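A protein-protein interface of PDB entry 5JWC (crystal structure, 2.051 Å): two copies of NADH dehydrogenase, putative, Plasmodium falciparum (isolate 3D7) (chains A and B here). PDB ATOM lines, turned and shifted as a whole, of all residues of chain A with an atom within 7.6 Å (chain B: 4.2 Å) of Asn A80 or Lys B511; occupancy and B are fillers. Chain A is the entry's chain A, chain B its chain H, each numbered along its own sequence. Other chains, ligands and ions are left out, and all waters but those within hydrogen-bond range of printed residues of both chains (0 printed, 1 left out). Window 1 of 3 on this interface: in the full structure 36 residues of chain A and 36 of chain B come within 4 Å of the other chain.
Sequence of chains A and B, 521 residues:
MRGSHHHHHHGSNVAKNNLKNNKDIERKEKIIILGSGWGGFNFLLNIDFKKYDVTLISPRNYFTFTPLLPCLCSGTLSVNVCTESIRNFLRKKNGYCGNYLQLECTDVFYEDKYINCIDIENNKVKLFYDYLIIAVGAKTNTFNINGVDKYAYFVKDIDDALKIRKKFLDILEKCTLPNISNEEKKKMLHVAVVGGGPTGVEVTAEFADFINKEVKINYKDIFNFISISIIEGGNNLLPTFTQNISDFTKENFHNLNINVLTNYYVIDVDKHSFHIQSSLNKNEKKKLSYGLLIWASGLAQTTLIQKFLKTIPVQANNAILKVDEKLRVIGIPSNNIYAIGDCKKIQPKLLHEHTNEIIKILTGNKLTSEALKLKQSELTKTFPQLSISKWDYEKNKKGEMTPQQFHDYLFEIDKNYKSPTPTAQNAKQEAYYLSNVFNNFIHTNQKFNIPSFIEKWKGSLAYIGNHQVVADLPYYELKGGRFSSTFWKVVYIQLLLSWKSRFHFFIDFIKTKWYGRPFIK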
ATOM      1  N   LEU A  72       5.445  -0.485 -26.660  1.00  0.00           N
ATOM      2  CA  LEU A  72       5.613   0.435 -27.766  1.00  0.00           C
ATOM      3  C   LEU A  72       4.334   1.219 -28.044  1.00  0.00           C
ATOM      4  O   LEU A  72       4.401   2.399 -28.407  1.00  0.00           O
ATOM      5  CB  LEU A  72       6.048  -0.349 -29.008  1.00  0.00           C
ATOM      6  CG  LEU A  72       7.008   0.203 -30.038  1.00  0.00           C
ATOM      7  CD1 LEU A  72       8.242   0.854 -29.409  1.00  0.00           C
ATOM      8  CD2 LEU A  72       7.396  -0.958 -30.977  1.00  0.00           C
ATOM      9  N   LEU A  77       8.521   1.918 -23.969  1.00  0.00           N
ATOM     10  CA  LEU A  77       9.828   1.560 -24.512  1.00  0.00           C
ATOM     11  C   LEU A  77       9.881   2.007 -25.970  1.00  0.00           C
ATOM     12  O   LEU A  77       8.841   2.209 -26.579  1.00  0.00           O
ATOM     13  CB  LEU A  77      10.066   0.056 -24.410  1.00  0.00           C
ATOM     14  CG  LEU A  77      10.083  -0.535 -23.007  1.00  0.00           C
ATOM     15  CD1 LEU A  77      10.170  -2.060 -23.108  1.00  0.00           C
ATOM     16  CD2 LEU A  77      11.254   0.017 -22.224  1.00  0.00           C
ATOM     17  N   SER A  78      11.079   2.137 -26.531  1.00  0.00           N
ATOM     18  CA  SER A  78      11.231   2.593 -27.911  1.00  0.00           C
ATOM     19  C   SER A  78      11.573   1.454 -28.881  1.00  0.00           C
ATOM     20  O   SER A  78      11.831   0.309 -28.482  1.00  0.00           O
ATOM     21  CB  SER A  78      12.317   3.668 -27.997  1.00  0.00           C
ATOM     22  OG  SER A  78      13.573   3.133 -27.605  1.00  0.00           O
ATOM     23  N   VAL A  79      11.578   1.781 -30.168  1.00  0.00           N
ATOM     24  CA  VAL A  79      11.837   0.795 -31.188  1.00  0.00           C
ATOM     25  C   VAL A  79      13.231   0.178 -31.055  1.00  0.00           C
ATOM     26  O   VAL A  79      13.416  -0.988 -31.391  1.00  0.00           O
ATOM     27  CB  VAL A  79      11.637   1.406 -32.589  1.00  0.00           C
ATOM     28  CG1 VAL A  79      12.116   0.458 -33.694  1.00  0.00           C
ATOM     29  CG2 VAL A  79      10.168   1.699 -32.788  1.00  0.00           C
ATOM     30  N   ASN A  80      14.208   0.934 -30.562  1.00  0.00           N
ATOM     31  CA  ASN A  80      15.559   0.363 -30.411  1.00  0.00           C
ATOM     32  C   ASN A  80      15.632  -0.791 -29.405  1.00  0.00           C
ATOM     33  O   ASN A  80      16.541  -1.635 -29.481  1.00  0.00           O
ATOM     34  CB  ASN A  80      16.567   1.458 -30.028  1.00  0.00           C
ATOM     35  CG  ASN A  80      16.804   2.451 -31.170  1.00  0.00           C
ATOM     36  OD1 ASN A  80      16.532   3.642 -31.043  1.00  0.00           O
ATOM     37  ND2 ASN A  80      17.280   1.943 -32.305  1.00  0.00           N
ATOM     38  N   VAL A  81      14.701  -0.823 -28.450  1.00  0.00           N
ATOM     39  CA  VAL A  81      14.635  -1.928 -27.492  1.00  0.00           C
ATOM     40  C   VAL A  81      14.035  -3.155 -28.147  1.00  0.00           C
ATOM     41  O   VAL A  81      14.406  -4.278 -27.816  1.00  0.00           O
ATOM     42  CB  VAL A  81      13.778  -1.590 -26.228  1.00  0.00           C
ATOM     43  CG1 VAL A  81      13.805  -2.753 -25.219  1.00  0.00           C
ATOM     44  CG2 VAL A  81      14.277  -0.337 -25.567  1.00  0.00           C
ATOM     45  N   CYS A  82      13.142  -2.936 -29.109  1.00  0.00           N
ATOM     46  CA  CYS A  82      12.291  -4.004 -29.632  1.00  0.00           C
ATOM     47  C   CYS A  82      12.732  -4.620 -30.962  1.00  0.00           C
ATOM     48  O   CYS A  82      12.019  -5.468 -31.514  1.00  0.00           O
ATOM     49  CB  CYS A  82      10.867  -3.478 -29.825  1.00  0.00           C
ATOM     50  SG  CYS A  82      10.078  -2.849 -28.377  1.00  0.00           S
ATOM     51  N   THR A  83      13.863  -4.179 -31.505  1.00  0.00           N
ATOM     52  CA  THR A  83      14.316  -4.696 -32.802  1.00  0.00           C
ATOM     53  C   THR A  83      15.794  -5.048 -32.801  1.00  0.00           C
ATOM     54  O   THR A  83      16.568  -4.575 -31.957  1.00  0.00           O
ATOM     55  CB  THR A  83      14.092  -3.681 -33.949  1.00  0.00           C
ATOM     56  OG1 THR A  83      14.621  -2.419 -33.552  1.00  0.00           O
ATOM     57  CG2 THR A  83      12.612  -3.493 -34.281  1.00  0.00           C
ATOM     58  N   GLU A  84      16.168  -5.899 -33.749  1.00  0.00           N
ATOM     59  CA  GLU A  84      17.573  -6.137 -34.084  1.00  0.00           C
ATOM     60  C   GLU A  84      17.695  -6.158 -35.603  1.00  0.00           C
ATOM     61  O   GLU A  84      16.910  -6.828 -36.276  1.00  0.00           O
ATOM     62  CB  GLU A  84      18.087  -7.471 -33.526  1.00  0.00           C
ATOM     63  CG  GLU A  84      17.896  -7.682 -32.037  1.00  0.00           C
ATOM     64  CD  GLU A  84      18.853  -6.847 -31.197  1.00  0.00           C
ATOM     65  OE1 GLU A  84      18.821  -6.961 -29.951  1.00  0.00           O
ATOM     66  OE2 GLU A  84      19.638  -6.081 -31.781  1.00  0.00           O
ATOM     67  N   ILE A 158       6.113  -4.225 -35.248  1.00  0.00           N
ATOM     68  CA  ILE A 158       6.503  -2.871 -34.888  1.00  0.00           C
ATOM     69  C   ILE A 158       5.563  -1.829 -35.502  1.00  0.00           C
ATOM     70  O   ILE A 158       5.076  -0.934 -34.800  1.00  0.00           O
ATOM     71  CB  ILE A 158       7.946  -2.588 -35.339  1.00  0.00           C
ATOM     72  CG1 ILE A 158       8.907  -3.576 -34.672  1.00  0.00           C
ATOM     73  CG2 ILE A 158       8.330  -1.151 -35.017  1.00  0.00           C
ATOM     74  CD1 ILE A 158       9.053  -3.379 -33.185  1.00  0.00           C
ATOM     75  N   LEU A 496      16.662 -10.119 -23.731  1.00  0.00           N
ATOM     76  CA  LEU A 496      17.054  -9.327 -24.893  1.00  0.00           C
ATOM     77  C   LEU A 496      18.318  -9.932 -25.555  1.00  0.00           C
ATOM     78  O   LEU A 496      19.153 -10.504 -24.876  1.00  0.00           O
ATOM     79  CB  LEU A 496      17.271  -7.869 -24.478  1.00  0.00           C
ATOM     80  CG  LEU A 496      15.992  -7.108 -24.132  1.00  0.00           C
ATOM     81  CD1 LEU A 496      16.332  -5.743 -23.529  1.00  0.00           C
ATOM     82  CD2 LEU A 496      15.075  -6.957 -25.378  1.00  0.00           C
ATOM     83  N   SER A 498      20.882  -8.619 -27.462  1.00  0.00           N
ATOM     84  CA  SER A 498      22.123  -7.876 -27.669  1.00  0.00           C
ATOM     85  C   SER A 498      22.332  -6.863 -26.554  1.00  0.00           C
ATOM     86  O   SER A 498      21.373  -6.447 -25.900  1.00  0.00           O
ATOM     87  CB  SER A 498      22.121  -7.155 -29.017  1.00  0.00           C
ATOM     88  OG  SER A 498      21.202  -6.083 -28.997  1.00  0.00           O
ATOM     89  N   LYS A 500      23.264  -3.796 -27.126  1.00  0.00           N
ATOM     90  CA  LYS A 500      22.618  -2.590 -27.641  1.00  0.00           C
ATOM     91  C   LYS A 500      21.171  -2.481 -27.112  1.00  0.00           C
ATOM     92  O   LYS A 500      20.761  -1.450 -26.590  1.00  0.00           O
ATOM     93  CB  LYS A 500      22.624  -2.596 -29.188  1.00  0.00           C
ATOM     94  CG  LYS A 500      21.985  -1.362 -29.851  1.00  0.00           C
ATOM     95  CD  LYS A 500      20.474  -1.539 -30.086  1.00  0.00           C
ATOM     96  CE  LYS A 500      20.176  -2.731 -31.009  1.00  0.00           C
ATOM     97  NZ  LYS A 500      18.700  -3.006 -31.099  1.00  0.00           N
ATOM     98  N   SER A 501      20.404  -3.551 -27.262  1.00  0.00           N
ATOM     99  CA  SER A 501      19.013  -3.529 -26.823  1.00  0.00           C
ATOM    100  C   SER A 501      18.911  -3.366 -25.306  1.00  0.00           C
ATOM    101  O   SER A 501      18.003  -2.704 -24.813  1.00  0.00           O
ATOM    102  CB  SER A 501      18.300  -4.794 -27.270  1.00  0.00           C
ATOM    103  OG  SER A 501      18.197  -4.799 -28.684  1.00  0.00           O
ATOM    104  N   ARG A 502      19.833  -3.977 -24.578  1.00  0.00           N
ATOM    105  CA  ARG A 502      19.843  -3.877 -23.123  1.00  0.00           C
ATOM    106  C   ARG A 502      20.163  -2.454 -22.690  1.00  0.00           C
ATOM    107  O   ARG A 502      19.595  -1.939 -21.720  1.00  0.00           O
ATOM    108  CB  ARG A 502      20.864  -4.852 -22.520  1.00  0.00           C
ATOM    109  CG  ARG A 502      20.452  -6.300 -22.673  1.00  0.00           C
ATOM    110  CD  ARG A 502      21.515  -7.274 -22.165  1.00  0.00           C
ATOM    111  NE  ARG A 502      21.106  -8.649 -22.452  1.00  0.00           N
ATOM    112  CZ  ARG A 502      21.928  -9.694 -22.522  1.00  0.00           C
ATOM    113  NH1 ARG A 502      23.227  -9.547 -22.306  1.00  0.00           N
ATOM    114  NH2 ARG A 502      21.436 -10.897 -22.790  1.00  0.00           N
ATOM    115  N   PHE A 503      21.098  -1.838 -23.410  1.00  0.00           N
ATOM    116  CA  PHE A 503      21.440  -0.435 -23.206  1.00  0.00           C
ATOM    117  C   PHE A 503      20.168   0.418 -23.335  1.00  0.00           C
ATOM    118  O   PHE A 503      19.798   1.164 -22.429  1.00  0.00           O
ATOM    119  CB  PHE A 503      22.502  -0.002 -24.236  1.00  0.00           C
ATOM    120  CG  PHE A 503      22.826   1.469 -24.199  1.00  0.00           C
ATOM    121  CD1 PHE A 503      23.732   1.964 -23.286  1.00  0.00           C
ATOM    122  CD2 PHE A 503      22.204   2.356 -25.073  1.00  0.00           C
ATOM    123  CE1 PHE A 503      24.033   3.327 -23.246  1.00  0.00           C
ATOM    124  CE2 PHE A 503      22.502   3.714 -25.039  1.00  0.00           C
ATOM    125  CZ  PHE A 503      23.415   4.194 -24.119  1.00  0.00           C
ATOM    126  N   HIS A 504      19.453   0.249 -24.439  1.00  0.00           N
ATOM    127  CA  HIS A 504      18.223   1.011 -24.661  1.00  0.00           C
ATOM    128  C   HIS A 504      17.121   0.697 -23.638  1.00  0.00           C
ATOM    129  O   HIS A 504      16.391   1.592 -23.196  1.00  0.00           O
ATOM    130  CB  HIS A 504      17.710   0.764 -26.073  1.00  0.00           C
ATOM    131  CG  HIS A 504      18.471   1.516 -27.116  1.00  0.00           C
ATOM    132  ND1 HIS A 504      18.229   2.845 -27.385  1.00  0.00           N
ATOM    133  CD2 HIS A 504      19.454   1.128 -27.965  1.00  0.00           C
ATOM    134  CE1 HIS A 504      19.038   3.246 -28.357  1.00  0.00           C
ATOM    135  NE2 HIS A 504      19.785   2.225 -28.726  1.00  0.00           N
ATOM    136  N   PHE A 505      17.014  -0.574 -23.270  1.00  0.00           N
ATOM    137  CA  PHE A 505      16.057  -1.004 -22.242  1.00  0.00           C
ATOM    138  C   PHE A 505      16.244  -0.180 -20.957  1.00  0.00           C
ATOM    139  O   PHE A 505      15.293   0.361 -20.390  1.00  0.00           O
ATOM    140  CB  PHE A 505      16.259  -2.491 -21.968  1.00  0.00           C
ATOM    141  CG  PHE A 505      15.196  -3.131 -21.110  1.00  0.00           C
ATOM    142  CD1 PHE A 505      13.943  -3.427 -21.625  1.00  0.00           C
ATOM    143  CD2 PHE A 505      15.485  -3.520 -19.816  1.00  0.00           C
ATOM    144  CE1 PHE A 505      12.986  -4.070 -20.838  1.00  0.00           C
ATOM    145  CE2 PHE A 505      14.531  -4.162 -19.025  1.00  0.00           C
ATOM    146  CZ  PHE A 505      13.289  -4.438 -19.537  1.00  0.00           C
ATOM    147  N   ILE A 507      18.011   2.713 -20.608  1.00  0.00           N
ATOM    148  CA  ILE A 507      17.881   4.152 -20.867  1.00  0.00           C
ATOM    149  C   ILE A 507      16.412   4.564 -20.952  1.00  0.00           C
ATOM    150  O   ILE A 507      16.009   5.597 -20.404  1.00  0.00           O
ATOM    151  CB  ILE A 507      18.588   4.569 -22.180  1.00  0.00           C
ATOM    152  CG1 ILE A 507      20.109   4.405 -22.062  1.00  0.00           C
ATOM    153  CG2 ILE A 507      18.205   6.014 -22.590  1.00  0.00           C
ATOM    154  CD1 ILE A 507      20.720   5.079 -20.842  1.00  0.00           C
ATOM    155  N   ASP A 508      15.608   3.748 -21.630  1.00  0.00           N
ATOM    156  CA  ASP A 508      14.193   4.050 -21.771  1.00  0.00           C
ATOM    157  C   ASP A 508      13.479   4.149 -20.425  1.00  0.00           C
ATOM    158  O   ASP A 508      12.599   4.992 -20.249  1.00  0.00           O
ATOM    159  CB  ASP A 508      13.499   2.998 -22.644  1.00  0.00           C
ATOM    160  CG  ASP A 508      13.650   3.290 -24.132  1.00  0.00           C
ATOM    161  OD1 ASP A 508      14.268   4.329 -24.483  1.00  0.00           O
ATOM    162  OD2 ASP A 508      13.137   2.491 -24.950  1.00  0.00           O
ATOM    163  N   ILE B 507      23.089  10.743 -24.771  1.00  0.00           N
ATOM    164  CA  ILE B 507      22.896   9.296 -24.930  1.00  0.00           C
ATOM    165  C   ILE B 507      23.109   8.855 -26.381  1.00  0.00           C
ATOM    166  O   ILE B 507      23.740   7.822 -26.637  1.00  0.00           O
ATOM    167  CB  ILE B 507      21.487   8.858 -24.473  1.00  0.00           C
ATOM    168  CG1 ILE B 507      21.344   9.019 -22.961  1.00  0.00           C
ATOM    169  CG2 ILE B 507      21.188   7.401 -24.896  1.00  0.00           C
ATOM    170  CD1 ILE B 507      22.442   8.358 -22.177  1.00  0.00           C
ATOM    171  N   ASP B 508      22.592   9.636 -27.330  1.00  0.00           N
ATOM    172  CA  ASP B 508      22.753   9.306 -28.736  1.00  0.00           C
ATOM    173  C   ASP B 508      24.221   9.236 -29.145  1.00  0.00           C
ATOM    174  O   ASP B 508      24.597   8.403 -29.953  1.00  0.00           O
ATOM    175  CB  ASP B 508      22.029  10.319 -29.632  1.00  0.00           C
ATOM    176  CG  ASP B 508      20.554   9.997 -29.789  1.00  0.00           C
ATOM    177  OD1 ASP B 508      20.107   8.971 -29.226  1.00  0.00           O
ATOM    178  OD2 ASP B 508      19.847  10.759 -30.483  1.00  0.00           O
ATOM    179  N   PHE B 509      25.062  10.110 -28.603  1.00  0.00           N
ATOM    180  CA  PHE B 509      26.469  10.005 -28.960  1.00  0.00           C
ATOM    181  C   PHE B 509      27.118   8.780 -28.331  1.00  0.00           C
ATOM    182  O   PHE B 509      27.916   8.112 -28.990  1.00  0.00           O
ATOM    183  CB  PHE B 509      27.209  11.290 -28.609  1.00  0.00           C
ATOM    184  CG  PHE B 509      27.058  12.349 -29.673  1.00  0.00           C
ATOM    185  CD1 PHE B 509      27.541  12.112 -30.956  1.00  0.00           C
ATOM    186  CD2 PHE B 509      26.409  13.545 -29.413  1.00  0.00           C
ATOM    187  CE1 PHE B 509      27.397  13.045 -31.951  1.00  0.00           C
ATOM    188  CE2 PHE B 509      26.267  14.483 -30.398  1.00  0.00           C
ATOM    189  CZ  PHE B 509      26.763  14.233 -31.678  1.00  0.00           C
ATOM    190  N   ILE B 510      26.770   8.464 -27.086  1.00  0.00           N
ATOM    191  CA  ILE B 510      27.206   7.200 -26.491  1.00  0.00           C
ATOM    192  C   ILE B 510      26.744   6.011 -27.338  1.00  0.00           C
ATOM    193  O   ILE B 510      27.532   5.109 -27.642  1.00  0.00           O
ATOM    194  CB  ILE B 510      26.684   7.013 -25.054  1.00  0.00           C
ATOM    195  CG1 ILE B 510      27.196   8.127 -24.141  1.00  0.00           C
ATOM    196  CG2 ILE B 510      27.118   5.643 -24.501  1.00  0.00           C
ATOM    197  CD1 ILE B 510      28.703   8.162 -24.039  1.00  0.00           C
ATOM    198  N   LYS B 511      25.465   6.023 -27.711  1.00  0.00           N
ATOM    199  CA  LYS B 511      24.865   4.936 -28.473  1.00  0.00           C
ATOM    200  C   LYS B 511      25.602   4.723 -29.790  1.00  0.00           C
ATOM    201  O   LYS B 511      25.928   3.598 -30.168  1.00  0.00           O
ATOM    202  CB  LYS B 511      23.374   5.231 -28.734  1.00  0.00           C
ATOM    203  CG  LYS B 511      22.607   4.124 -29.466  1.00  0.00           C
ATOM    204  CD  LYS B 511      22.648   4.296 -30.989  1.00  0.00           C
ATOM    205  CE  LYS B 511      22.093   3.055 -31.704  1.00  0.00           C
ATOM    206  NZ  LYS B 511      20.632   2.837 -31.485  1.00  0.00           N
ATOM    207  N   THR B 512      25.823   5.819 -30.497  1.00  0.00           N
ATOM    208  CA  THR B 512      26.445   5.785 -31.808  1.00  0.00           C
ATOM    209  C   THR B 512      27.907   5.319 -31.714  1.00  0.00           C
ATOM    210  O   THR B 512      28.371   4.539 -32.546  1.00  0.00           O
ATOM    211  CB  THR B 512      26.332   7.162 -32.469  1.00  0.00           C
ATOM    212  OG1 THR B 512      24.960   7.357 -32.842  1.00  0.00           O
ATOM    213  CG2 THR B 512      27.168   7.248 -33.712  1.00  0.00           C
ATOM    214  N   LYS B 513      28.619   5.769 -30.683  1.00  0.00           N
ATOM    215  CA  LYS B 513      29.998   5.316 -30.495  1.00  0.00           C
ATOM    216  C   LYS B 513      30.104   3.818 -30.194  1.00  0.00           C
ATOM    217  O   LYS B 513      30.978   3.137 -30.712  1.00  0.00           O
ATOM    218  CB  LYS B 513      30.668   6.091 -29.367  1.00  0.00           C
ATOM    219  CG  LYS B 513      32.180   5.815 -29.261  1.00  0.00           C
ATOM    220  CD  LYS B 513      32.793   6.613 -28.116  1.00  0.00           C
ATOM    221  CE  LYS B 513      34.258   6.270 -27.901  1.00  0.00           C
ATOM    222  NZ  LYS B 513      34.799   7.125 -26.806  1.00  0.00           N
ATOM    223  N   TRP B 514      29.226   3.310 -29.337  1.00  0.00           N
ATOM    224  CA  TRP B 514      29.309   1.916 -28.893  1.00  0.00           C
ATOM    225  C   TRP B 514      28.661   0.913 -29.834  1.00  0.00           C
ATOM    226  O   TRP B 514      29.141  -0.206 -29.969  1.00  0.00           O
ATOM    227  CB  TRP B 514      28.647   1.742 -27.519  1.00  0.00           C
ATOM    228  CG  TRP B 514      29.361   2.374 -26.381  1.00  0.00           C
ATOM    229  CD1 TRP B 514      30.500   3.112 -26.435  1.00  0.00           C
ATOM    230  CD2 TRP B 514      28.971   2.320 -25.002  1.00  0.00           C
ATOM    231  NE1 TRP B 514      30.857   3.518 -25.169  1.00  0.00           N
ATOM    232  CE2 TRP B 514      29.933   3.049 -24.272  1.00  0.00           C
ATOM    233  CE3 TRP B 514      27.907   1.724 -24.311  1.00  0.00           C
ATOM    234  CZ2 TRP B 514      29.859   3.201 -22.883  1.00  0.00           C
ATOM    235  CZ3 TRP B 514      27.838   1.871 -22.927  1.00  0.00           C
ATOM    236  CH2 TRP B 514      28.807   2.605 -22.232  1.00  0.00           C
ATOM    237  N   TYR B 515      27.540   1.283 -30.446  1.00  0.00           N
ATOM    238  CA  TYR B 515      26.780   0.307 -31.229  1.00  0.00           C
ATOM    239  C   TYR B 515      26.592   0.724 -32.674  1.00  0.00           C
ATOM    240  O   TYR B 515      26.068  -0.040 -33.465  1.00  0.00           O
ATOM    241  CB  TYR B 515      25.402   0.049 -30.588  1.00  0.00           C
ATOM    242  CG  TYR B 515      25.502  -0.273 -29.117  1.00  0.00           C
ATOM    243  CD1 TYR B 515      26.045  -1.481 -28.687  1.00  0.00           C
ATOM    244  CD2 TYR B 515      25.080   0.627 -28.162  1.00  0.00           C
ATOM    245  CE1 TYR B 515      26.157  -1.776 -27.351  1.00  0.00           C
ATOM    246  CE2 TYR B 515      25.194   0.334 -26.805  1.00  0.00           C
ATOM    247  CZ  TYR B 515      25.727  -0.863 -26.416  1.00  0.00           C
ATOM    248  OH  TYR B 515      25.832  -1.143 -25.078  1.00  0.00           O
ATOM    249  N   GLY B 516      26.987   1.947 -33.011  1.00  0.00           N
ATOM    250  CA  GLY B 516      26.844   2.436 -34.371  1.00  0.00           C
ATOM    251  C   GLY B 516      25.458   2.967 -34.699  1.00  0.00           C
ATOM    252  O   GLY B 516      24.526   2.829 -33.909  1.00  0.00           O
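The side-chain amino group of Lys B511 is in hydrogen-bond range of a ring nitrogen (NE2) of His A504, at 3.0 Å.
The backbone carbonyl oxygen (O) of Asn A80 sits at hydrogen-bond distance from the side-chain amino group (NZ) of Lys A500 (3.0 Å). The backbone carbonyl oxygen (O) of Thr A83 sits at hydrogen-bond distance from the side-chain amino group (NZ) of Lys A500. NZ of Lys A500 is in salt-bridge range of OE2 of Glu A84, at 3.3 Å. The side-chain amino group (NZ) of Lys A500 lies within hydrogen-bond range of the side-chain hydroxyl (OG) of Ser A501 (3.0 Å). The backbone carbonyl oxygen of Lys B511 lies within hydrogen-bond range of the backbone NH of Gly B516 (3.5 Å).
Lys B511 touches Asn A80. Tyr B515 touches Lys A500 (CE1 to N, 3.5 Å). Phe A503 touches Ile B507 (CE2 to CG2, 3.9 Å). Phe A503 touches Ile B510. Phe A503 touches Tyr B515 (CB to OH, 3.6 Å). CD1 of Ile A507 touches CD1 of Ile B507, 3.9 Å away.
Printed residues of chain B within 4 Å of Lys A500: Tyr B515. Of the printed residues of chain B, His A504 touches Lys B511 (3.0 Å). Printed residues of chain B within 4 Å of Ile A507: Ile B507 (3.9 Å). Lys B511 touches two residues of chain A. The nearest printed residue of chain B that does not touch Asn A80 is Asp B508 (6.7 Å). The nearest residue of chain A that does not touch Lys B511 is Phe A503 (4.1 Å). The nearest printed residue of chain A that does not touch Tyr B515 is His A504 (5.6 Å).
Printed residues of chain B that touch a printed residue of chain A: Ile B507, Ile B510, Lys B511 and Tyr B515. Of the 20 printed residues of chain A, 5 touch a printed residue of chain B. Hydrophobic or aromatic side chains of chain A within 4 Å of the printed part of chain B: Phe A503, His A504 and Ile A507. Among the printed residues, no Asp or Glu carboxylate lies within 4 Å of a Lys or Arg side-chain nitrogen of the other chain.
Ile B507 touches its own counterpart, Ile A507. Positions printed for both chains: 507 and 508. Of the 7 pairs that touch across the chains among the printed residues, 1 has its exchanged pair printed and touching as well.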
